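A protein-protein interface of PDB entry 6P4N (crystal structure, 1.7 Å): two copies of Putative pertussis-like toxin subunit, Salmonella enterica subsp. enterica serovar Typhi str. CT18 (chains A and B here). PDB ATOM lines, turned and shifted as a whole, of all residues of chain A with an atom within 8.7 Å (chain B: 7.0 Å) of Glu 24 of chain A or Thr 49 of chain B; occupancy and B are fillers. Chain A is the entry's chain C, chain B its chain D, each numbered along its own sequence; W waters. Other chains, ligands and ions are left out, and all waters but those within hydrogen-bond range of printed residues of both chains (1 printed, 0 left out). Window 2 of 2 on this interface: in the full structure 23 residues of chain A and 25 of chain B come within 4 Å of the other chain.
OE2 of Glu 24 of chain A sits at hydrogen-bond distance from NE2 of Gln 46 of chain B (2.8 Å).
The backbone carbonyl oxygen of Glu 24 of chain A sits at hydrogen-bond distance from the backbone NH of Asp 48 of chain B, 2.9 Å away.
The side-chain carboxylate (OE2) of Glu 24 of chain A lies within hydrogen-bond range of the backbone NH (N) of Thr 49 of chain B, 2.7 Å away.
The side-chain hydroxyl (OG1) of Thr 26 of chain A sits at hydrogen-bond distance from the backbone NH (N) of Gln 46 of chain B, 2.8 Å away.
O of Ile 77 of chain A lies within hydrogen-bond range of NE2 of Gln 46 of chain B, 2.8 Å away.
O of Trp 78 of chain A sits close to OE1 of Gln 46 of chain B, 3.2 Å away.
OE1 of Gln 46 of chain B sits at hydrogen-bond distance from OG of Ser 81 of chain A.
Water W1 lies within hydrogen-bond range of the side-chain carboxylate (OD1) of Asp 28 of chain A (2.6 Å) and the side-chain hydroxyl (OH) of Tyr 110 of chain B (2.6 Å).
Printed residues of chain B that touch a printed residue of chain A: Gln 46, Ile 47, Asp 48, Thr 49, Pro 51 and Tyr 110.
Hydrophobic or aromatic side chains of chain B within 4 Å of the printed part of chain A: Ile 47, Pro 51 and Tyr 110.
Along chain B the printed residues that touch a printed residue of chain A span positions 46 to 110.
Of the 17 printed residues of chain A, 8 touch a printed residue of chain B.
Printed residues of chain A that touch a printed residue of chain B: Glu 24, Trp 25, Thr 26, Ile 77, Trp 78, Pro 80, Ser 81 and Glu 84.
Hydrophobic or aromatic side chains of chain A that line the printed part of chain B: Trp 25, Trp 78 and Pro 80.
Among the printed residues, no Asp or Glu carboxylate lies within 4 Å of a Lys or Arg side-chain nitrogen of the other chain.
No position is printed for both chains.
Glu 24 of chain A touches just these residues of chain B: Gln 46, Ile 47, Asp 48 and Thr 49.
Of the printed residues of chain B, Thr 26 of chain A touches Gln 46 (2.8 Å).
Of the printed residues of chain B, Ser 81 of chain A touches Gln 46 (2.8 Å) and Pro 51 (3.3 Å).
Printed residues of chain B within 4 Å of Glu 84 of chain A: Pro 51 (3.7 Å).
Printed residues of chain A within 4 Å of Gln 46 of chain B: Glu 24, Trp 25, Thr 26, Ile 77, Trp 78, Pro 80 and Ser 81.
Of chain A, only Glu 24 (2.7 Å) and Pro 80 (3.3 Å) come within 4 Å of Thr 49 of chain B.
Printed residues of chain A within 4 Å of Pro 51 of chain B: Pro 80, Ser 81 and Glu 84.
The side-chain amide nitrogen of Asn 31 of chain A is in hydrogen-bond range of the backbone carbonyl oxygen of Trp 25 of chain A, 3.0 Å away.
The backbone carbonyl oxygen (O) of Thr 26 of chain A lies within hydrogen-bond range of the side-chain amide nitrogen (ND2) of Asn 31 of chain A, 3.1 Å away.
OG1 of Thr 26 of chain A sits at hydrogen-bond distance from O of Val 123 of chain A.
OG of Ser 76 of chain A sits close to N of Trp 78 of chain A, at 3.1 Å.
The indole nitrogen of Trp 78 of chain A sits at hydrogen-bond distance from the side-chain amide oxygen of Gln 104 of chain A (2.8 Å).
O of Thr 49 of chain B lies within hydrogen-bond range of NZ of Lys 74 of chain B.
Among the printed residues, pairs that only touch across the chains: Pro 80 of chain A with Thr 49 of chain B (3.3 Å), Ser 81 of chain A with Pro 51 of chain B (3.3 Å), Trp 25 of chain A with Gln 46 of chain B (3.4 Å), Glu 24 of chain A with Ile 47 of chain B (3.5 Å), Pro 80 of chain A with Gln 46 of chain B (3.6 Å), Glu 84 of chain A with Pro 51 of chain B (3.7 Å), Pro 80 of chain A with Pro 51 of chain B (3.8 Å), Trp 25 of chain A with Ile 47 of chain B (3.8 Å) and Trp 25 of chain A with Tyr 110 of chain B (3.9 Å).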
ATOM      1  N   GLU A  24      29.011  -4.563  -9.637  1.00  0.00           N
ATOM      2  CA  GLU A  24      27.846  -5.067 -10.348  1.00  0.00           C
ATOM      3  C   GLU A  24      27.887  -4.634 -11.800  1.00  0.00           C
ATOM      4  O   GLU A  24      28.531  -3.642 -12.132  1.00  0.00           O
ATOM      5  CB  GLU A  24      26.554  -4.569  -9.700  1.00  0.00           C
ATOM      6  CG  GLU A  24      26.023  -3.222 -10.224  1.00  0.00           C
ATOM      7  CD  GLU A  24      26.961  -2.038  -9.998  1.00  0.00           C
ATOM      8  OE1 GLU A  24      27.983  -2.173  -9.286  1.00  0.00           O
ATOM      9  OE2 GLU A  24      26.667  -0.943 -10.530  1.00  0.00           O
ATOM     10  N   TRP A  25      27.191  -5.376 -12.658  1.00  0.00           N
ATOM     11  CA  TRP A  25      27.175  -5.084 -14.085  1.00  0.00           C
ATOM     12  C   TRP A  25      25.882  -5.622 -14.671  1.00  0.00           C
ATOM     13  O   TRP A  25      25.441  -6.713 -14.304  1.00  0.00           O
ATOM     14  CB  TRP A  25      28.390  -5.714 -14.804  1.00  0.00           C
ATOM     15  CG  TRP A  25      28.399  -5.547 -16.303  1.00  0.00           C
ATOM     16  CD1 TRP A  25      28.026  -4.434 -17.012  1.00  0.00           C
ATOM     17  CD2 TRP A  25      28.796  -6.527 -17.282  1.00  0.00           C
ATOM     18  NE1 TRP A  25      28.160  -4.662 -18.364  1.00  0.00           N
ATOM     19  CE2 TRP A  25      28.637  -5.936 -18.557  1.00  0.00           C
ATOM     20  CE3 TRP A  25      29.272  -7.847 -17.203  1.00  0.00           C
ATOM     21  CZ2 TRP A  25      28.936  -6.615 -19.744  1.00  0.00           C
ATOM     22  CZ3 TRP A  25      29.564  -8.522 -18.377  1.00  0.00           C
ATOM     23  CH2 TRP A  25      29.396  -7.905 -19.638  1.00  0.00           C
ATOM     24  N   THR A  26      25.266  -4.841 -15.568  1.00  0.00           N
ATOM     25  CA  THR A  26      24.167  -5.327 -16.396  1.00  0.00           C
ATOM     26  C   THR A  26      24.397  -6.754 -16.879  1.00  0.00           C
ATOM     27  O   THR A  26      23.475  -7.575 -16.879  1.00  0.00           O
ATOM     28  CB  THR A  26      23.990  -4.395 -17.594  1.00  0.00           C
ATOM     29  OG1 THR A  26      23.630  -3.097 -17.108  1.00  0.00           O
ATOM     30  CG2 THR A  26      22.918  -4.930 -18.568  1.00  0.00           C
ATOM     31  N   GLY A  27      25.629  -7.054 -17.286  1.00  0.00           N
ATOM     32  CA  GLY A  27      25.944  -8.345 -17.857  1.00  0.00           C
ATOM     33  C   GLY A  27      26.280  -9.449 -16.881  1.00  0.00           C
ATOM     34  O   GLY A  27      26.661 -10.535 -17.332  1.00  0.00           O
ATOM     35  N   ASP A  28      26.144  -9.223 -15.570  1.00  0.00           N
ATOM     36  CA  ASP A  28      26.367 -10.299 -14.600  1.00  0.00           C
ATOM     37  C   ASP A  28      25.503 -11.512 -14.913  1.00  0.00           C
ATOM     38  O   ASP A  28      24.343 -11.388 -15.314  1.00  0.00           O
ATOM     39  CB  ASP A  28      26.063  -9.830 -13.178  1.00  0.00           C
ATOM     40  CG  ASP A  28      27.063  -8.838 -12.665  1.00  0.00           C
ATOM     41  OD1 ASP A  28      28.189  -8.812 -13.211  1.00  0.00           O
ATOM     42  OD2 ASP A  28      26.726  -8.096 -11.706  1.00  0.00           O
ATOM     43  N   THR A  30      24.164 -13.377 -12.860  1.00  0.00           N
ATOM     44  CA  THR A  30      23.052 -13.411 -11.924  1.00  0.00           C
ATOM     45  C   THR A  30      21.869 -12.571 -12.388  1.00  0.00           C
ATOM     46  O   THR A  30      20.806 -12.631 -11.759  1.00  0.00           O
ATOM     47  CB  THR A  30      23.513 -12.948 -10.542  1.00  0.00           C
ATOM     48  OG1 THR A  30      24.304 -11.761 -10.676  1.00  0.00           O
ATOM     49  CG2 THR A  30      24.360 -14.035  -9.876  1.00  0.00           C
ATOM     50  N   ASN A  31      22.019 -11.800 -13.462  1.00  0.00           N
ATOM     51  CA  ASN A  31      20.879 -11.123 -14.056  1.00  0.00           C
ATOM     52  C   ASN A  31      20.274 -12.013 -15.142  1.00  0.00           C
ATOM     53  O   ASN A  31      20.816 -13.064 -15.492  1.00  0.00           O
ATOM     54  CB  ASN A  31      21.303  -9.751 -14.597  1.00  0.00           C
ATOM     55  CG  ASN A  31      21.804  -8.826 -13.497  1.00  0.00           C
ATOM     56  OD1 ASN A  31      21.356  -8.901 -12.343  1.00  0.00           O
ATOM     57  ND2 ASN A  31      22.745  -7.959 -13.841  1.00  0.00           N
ATOM     58  N   SER A  76      17.466   0.828  -5.036  1.00  0.00           N
ATOM     59  CA  SER A  76      18.220  -0.329  -5.531  1.00  0.00           C
ATOM     60  C   SER A  76      19.596   0.095  -6.034  1.00  0.00           C
ATOM     61  O   SER A  76      19.873   1.288  -6.181  1.00  0.00           O
ATOM     62  CB  SER A  76      17.462  -1.088  -6.633  1.00  0.00           C
ATOM     63  OG  SER A  76      17.817  -0.611  -7.928  1.00  0.00           O
ATOM     64  N   ILE A  77      20.478  -0.885  -6.263  1.00  0.00           N
ATOM     65  CA  ILE A  77      21.827  -0.597  -6.727  1.00  0.00           C
ATOM     66  C   ILE A  77      21.819   0.006  -8.125  1.00  0.00           C
ATOM     67  O   ILE A  77      22.803   0.630  -8.531  1.00  0.00           O
ATOM     68  CB  ILE A  77      22.680  -1.882  -6.698  1.00  0.00           C
ATOM     69  CG1 ILE A  77      24.164  -1.541  -6.841  1.00  0.00           C
ATOM     70  CG2 ILE A  77      22.222  -2.853  -7.778  1.00  0.00           C
ATOM     71  CD1 ILE A  77      25.090  -2.741  -6.667  1.00  0.00           C
ATOM     72  N   TRP A  78      20.730  -0.170  -8.861  1.00  0.00           N
ATOM     73  CA  TRP A  78      20.604   0.325 -10.226  1.00  0.00           C
ATOM     74  C   TRP A  78      20.131   1.765 -10.288  1.00  0.00           C
ATOM     75  O   TRP A  78      19.997   2.306 -11.393  1.00  0.00           O
ATOM     76  CB  TRP A  78      19.645  -0.570 -11.017  1.00  0.00           C
ATOM     77  CG  TRP A  78      20.019  -2.008 -10.881  1.00  0.00           C
ATOM     78  CD1 TRP A  78      19.365  -2.954 -10.152  1.00  0.00           C
ATOM     79  CD2 TRP A  78      21.169  -2.650 -11.447  1.00  0.00           C
ATOM     80  NE1 TRP A  78      20.030  -4.157 -10.235  1.00  0.00           N
ATOM     81  CE2 TRP A  78      21.139  -3.994 -11.032  1.00  0.00           C
ATOM     82  CE3 TRP A  78      22.214  -2.219 -12.281  1.00  0.00           C
ATOM     83  CZ2 TRP A  78      22.115  -4.914 -11.416  1.00  0.00           C
ATOM     84  CZ3 TRP A  78      23.186  -3.132 -12.657  1.00  0.00           C
ATOM     85  CH2 TRP A  78      23.129  -4.465 -12.220  1.00  0.00           C
ATOM     86  N   ALA A  79      19.897   2.397  -9.134  1.00  0.00           N
ATOM     87  CA  ALA A  79      19.444   3.788  -9.115  1.00  0.00           C
ATOM     88  C   ALA A  79      20.254   4.731 -10.001  1.00  0.00           C
ATOM     89  O   ALA A  79      19.627   5.563 -10.685  1.00  0.00           O
ATOM     90  CB  ALA A  79      19.435   4.318  -7.672  1.00  0.00           C
ATOM     91  N   PRO A  80      21.597   4.678 -10.044  1.00  0.00           N
ATOM     92  CA  PRO A  80      22.334   5.659 -10.866  1.00  0.00           C
ATOM     93  C   PRO A  80      21.918   5.719 -12.325  1.00  0.00           C
ATOM     94  O   PRO A  80      22.052   6.783 -12.945  1.00  0.00           O
ATOM     95  CB  PRO A  80      23.790   5.199 -10.739  1.00  0.00           C
ATOM     96  CG  PRO A  80      23.847   4.509  -9.436  1.00  0.00           C
ATOM     97  CD  PRO A  80      22.532   3.827  -9.270  1.00  0.00           C
ATOM     98  N   SER A  81      21.427   4.627 -12.902  1.00  0.00           N
ATOM     99  CA  SER A  81      21.114   4.598 -14.325  1.00  0.00           C
ATOM    100  C   SER A  81      19.643   4.861 -14.606  1.00  0.00           C
ATOM    101  O   SER A  81      19.195   4.654 -15.739  1.00  0.00           O
ATOM    102  CB  SER A  81      21.537   3.257 -14.927  1.00  0.00           C
ATOM    103  OG  SER A  81      22.924   3.059 -14.738  1.00  0.00           O
ATOM    104  N   PHE A  82      18.888   5.321 -13.604  1.00  0.00           N
ATOM    105  CA  PHE A  82      17.457   5.540 -13.784  1.00  0.00           C
ATOM    106  C   PHE A  82      17.157   6.422 -14.995  1.00  0.00           C
ATOM    107  O   PHE A  82      16.349   6.057 -15.855  1.00  0.00           O
ATOM    108  CB  PHE A  82      16.857   6.164 -12.524  1.00  0.00           C
ATOM    109  CG  PHE A  82      15.409   6.532 -12.687  1.00  0.00           C
ATOM    110  CD1 PHE A  82      14.417   5.578 -12.547  1.00  0.00           C
ATOM    111  CD2 PHE A  82      15.044   7.836 -12.997  1.00  0.00           C
ATOM    112  CE1 PHE A  82      13.074   5.921 -12.720  1.00  0.00           C
ATOM    113  CE2 PHE A  82      13.723   8.169 -13.169  1.00  0.00           C
ATOM    114  CZ  PHE A  82      12.738   7.209 -13.033  1.00  0.00           C
ATOM    115  N   GLU A  84      19.070   7.360 -17.585  1.00  0.00           N
ATOM    116  CA  GLU A  84      19.530   6.815 -18.863  1.00  0.00           C
ATOM    117  C   GLU A  84      18.604   5.712 -19.363  1.00  0.00           C
ATOM    118  O   GLU A  84      18.319   5.623 -20.565  1.00  0.00           O
ATOM    119  CB  GLU A  84      20.962   6.287 -18.722  1.00  0.00           C
ATOM    120  CG  GLU A  84      22.022   7.374 -18.675  1.00  0.00           C
ATOM    121  CD  GLU A  84      22.135   8.047 -17.310  1.00  0.00           C
ATOM    122  OE1 GLU A  84      21.480   7.603 -16.329  1.00  0.00           O
ATOM    123  OE2 GLU A  84      22.884   9.038 -17.226  1.00  0.00           O
ATOM    124  N   GLN A 104      17.117  -7.657 -13.229  1.00  0.00           N
ATOM    125  CA  GLN A 104      17.494  -8.417 -12.049  1.00  0.00           C
ATOM    126  C   GLN A 104      16.220  -8.769 -11.293  1.00  0.00           C
ATOM    127  O   GLN A 104      15.403  -7.891 -10.991  1.00  0.00           O
ATOM    128  CB  GLN A 104      18.476  -7.662 -11.150  1.00  0.00           C
ATOM    129  CG  GLN A 104      18.823  -8.498  -9.894  1.00  0.00           C
ATOM    130  CD  GLN A 104      19.888  -7.882  -9.014  1.00  0.00           C
ATOM    131  OE1 GLN A 104      19.999  -6.662  -8.899  1.00  0.00           O
ATOM    132  NE2 GLN A 104      20.667  -8.737  -8.352  1.00  0.00           N
ATOM    133  N   VAL A 123      17.742  -3.344 -15.823  1.00  0.00           N
ATOM    134  CA  VAL A 123      19.166  -3.069 -15.646  1.00  0.00           C
ATOM    135  C   VAL A 123      19.897  -2.843 -16.969  1.00  0.00           C
ATOM    136  O   VAL A 123      21.084  -2.482 -16.973  1.00  0.00           O
ATOM    137  CB  VAL A 123      19.850  -4.193 -14.835  1.00  0.00           C
ATOM    138  CG1 VAL A 123      19.038  -4.508 -13.595  1.00  0.00           C
ATOM    139  CG2 VAL A 123      20.038  -5.464 -15.672  1.00  0.00           C
ATOM    140  N   GLN B  46      24.567  -0.466 -16.797  1.00  0.00           N
ATOM    141  CA  GLN B  46      25.266   0.074 -15.641  1.00  0.00           C
ATOM    142  C   GLN B  46      26.428  -0.839 -15.275  1.00  0.00           C
ATOM    143  O   GLN B  46      26.308  -2.065 -15.358  1.00  0.00           O
ATOM    144  CB  GLN B  46      24.322   0.223 -14.430  1.00  0.00           C
ATOM    145  CG  GLN B  46      24.978   0.873 -13.218  1.00  0.00           C
ATOM    146  CD  GLN B  46      24.006   1.113 -12.086  1.00  0.00           C
ATOM    147  OE1 GLN B  46      22.996   1.801 -12.254  1.00  0.00           O
ATOM    148  NE2 GLN B  46      24.309   0.556 -10.911  1.00  0.00           N
ATOM    149  N   ILE B  47      27.546  -0.242 -14.867  1.00  0.00           N
ATOM    150  CA  ILE B  47      28.682  -1.009 -14.358  1.00  0.00           C
ATOM    151  C   ILE B  47      29.352  -0.226 -13.235  1.00  0.00           C
ATOM    152  O   ILE B  47      29.642   0.969 -13.378  1.00  0.00           O
ATOM    153  CB  ILE B  47      29.689  -1.362 -15.473  1.00  0.00           C
ATOM    154  CG1 ILE B  47      30.714  -2.380 -14.951  1.00  0.00           C
ATOM    155  CG2 ILE B  47      30.369  -0.123 -16.023  1.00  0.00           C
ATOM    156  CD1 ILE B  47      31.577  -2.998 -16.040  1.00  0.00           C
ATOM    157  N   ASP B  48      29.577  -0.900 -12.105  1.00  0.00           N
ATOM    158  CA  ASP B  48      30.287  -0.320 -10.966  1.00  0.00           C
ATOM    159  C   ASP B  48      29.729   1.057 -10.597  1.00  0.00           C
ATOM    160  O   ASP B  48      30.462   2.040 -10.456  1.00  0.00           O
ATOM    161  CB  ASP B  48      31.789  -0.256 -11.251  1.00  0.00           C
ATOM    162  CG  ASP B  48      32.403  -1.638 -11.423  1.00  0.00           C
ATOM    163  OD1 ASP B  48      31.974  -2.575 -10.714  1.00  0.00           O
ATOM    164  OD2 ASP B  48      33.313  -1.784 -12.265  1.00  0.00           O
ATOM    165  N   THR B  49      28.402   1.106 -10.444  1.00  0.00           N
ATOM    166  CA  THR B  49      27.584   2.258 -10.054  1.00  0.00           C
ATOM    167  C   THR B  49      27.499   3.335 -11.132  1.00  0.00           C
ATOM    168  O   THR B  49      26.973   4.427 -10.859  1.00  0.00           O
ATOM    169  CB  THR B  49      28.037   2.926  -8.740  1.00  0.00           C
ATOM    170  OG1 THR B  49      29.125   3.828  -8.988  1.00  0.00           O
ATOM    171  CG2 THR B  49      28.438   1.897  -7.697  1.00  0.00           C
ATOM    172  N   SER B  50      27.972   3.066 -12.347  1.00  0.00           N
ATOM    173  CA  SER B  50      27.985   4.083 -13.385  1.00  0.00           C
ATOM    174  C   SER B  50      27.116   3.671 -14.565  1.00  0.00           C
ATOM    175  O   SER B  50      27.295   2.568 -15.105  1.00  0.00           O
ATOM    176  CB  SER B  50      29.413   4.342 -13.883  1.00  0.00           C
ATOM    177  OG  SER B  50      29.383   5.267 -14.954  1.00  0.00           O
ATOM    178  N   PRO B  51      26.203   4.522 -15.021  1.00  0.00           N
ATOM    179  CA  PRO B  51      25.583   4.266 -16.321  1.00  0.00           C
ATOM    180  C   PRO B  51      26.655   4.256 -17.401  1.00  0.00           C
ATOM    181  O   PRO B  51      27.698   4.901 -17.280  1.00  0.00           O
ATOM    182  CB  PRO B  51      24.596   5.428 -16.503  1.00  0.00           C
ATOM    183  CG  PRO B  51      24.876   6.393 -15.426  1.00  0.00           C
ATOM    184  CD  PRO B  51      25.645   5.700 -14.341  1.00  0.00           C
ATOM    185  N   LYS B  74      31.058   7.664 -15.173  1.00  0.00           N
ATOM    186  CA  LYS B  74      31.898   8.004 -14.030  1.00  0.00           C
ATOM    187  C   LYS B  74      33.369   7.660 -14.224  1.00  0.00           C
ATOM    188  O   LYS B  74      34.158   7.854 -13.295  1.00  0.00           O
ATOM    189  CB  LYS B  74      31.374   7.312 -12.767  1.00  0.00           C
ATOM    190  CG  LYS B  74      29.980   7.762 -12.340  1.00  0.00           C
ATOM    191  CD  LYS B  74      29.482   6.960 -11.132  1.00  0.00           C
ATOM    192  CE  LYS B  74      28.056   7.369 -10.746  1.00  0.00           C
ATOM    193  NZ  LYS B  74      27.526   6.597  -9.568  1.00  0.00           N
ATOM    194  N   GLN B  75      33.767   7.167 -15.392  1.00  0.00           N
ATOM    195  CA  GLN B  75      35.102   6.609 -15.558  1.00  0.00           C
ATOM    196  C   GLN B  75      35.803   7.231 -16.757  1.00  0.00           C
ATOM    197  O   GLN B  75      35.164   7.648 -17.727  1.00  0.00           O
ATOM    198  CB  GLN B  75      35.054   5.082 -15.725  1.00  0.00           C
ATOM    199  CG  GLN B  75      34.496   4.334 -14.517  1.00  0.00           C
ATOM    200  CD  GLN B  75      34.523   2.833 -14.707  1.00  0.00           C
ATOM    201  OE1 GLN B  75      35.257   2.314 -15.550  1.00  0.00           O
ATOM    202  NE2 GLN B  75      33.710   2.123 -13.931  1.00  0.00           N
ATOM    203  N   TYR B 110      37.616  -4.239 -17.487  1.00  0.00           N
ATOM    204  CA  TYR B 110      36.892  -5.398 -16.976  1.00  0.00           C
ATOM    205  C   TYR B 110      36.793  -6.446 -18.077  1.00  0.00           C
ATOM    206  O   TYR B 110      36.169  -6.185 -19.114  1.00  0.00           O
ATOM    207  CB  TYR B 110      35.500  -5.008 -16.483  1.00  0.00           C
ATOM    208  CG  TYR B 110      34.754  -6.148 -15.831  1.00  0.00           C
ATOM    209  CD1 TYR B 110      35.355  -6.915 -14.842  1.00  0.00           C
ATOM    210  CD2 TYR B 110      33.454  -6.464 -16.208  1.00  0.00           C
ATOM    211  CE1 TYR B 110      34.685  -7.961 -14.241  1.00  0.00           C
ATOM    212  CE2 TYR B 110      32.771  -7.511 -15.606  1.00  0.00           C
ATOM    213  CZ  TYR B 110      33.395  -8.257 -14.624  1.00  0.00           C
ATOM    214  OH  TYR B 110      32.731  -9.302 -14.019  1.00  0.00           O
HETATM  215  O   HOH W   1      30.209  -9.968 -14.472  1.00  0.00           O
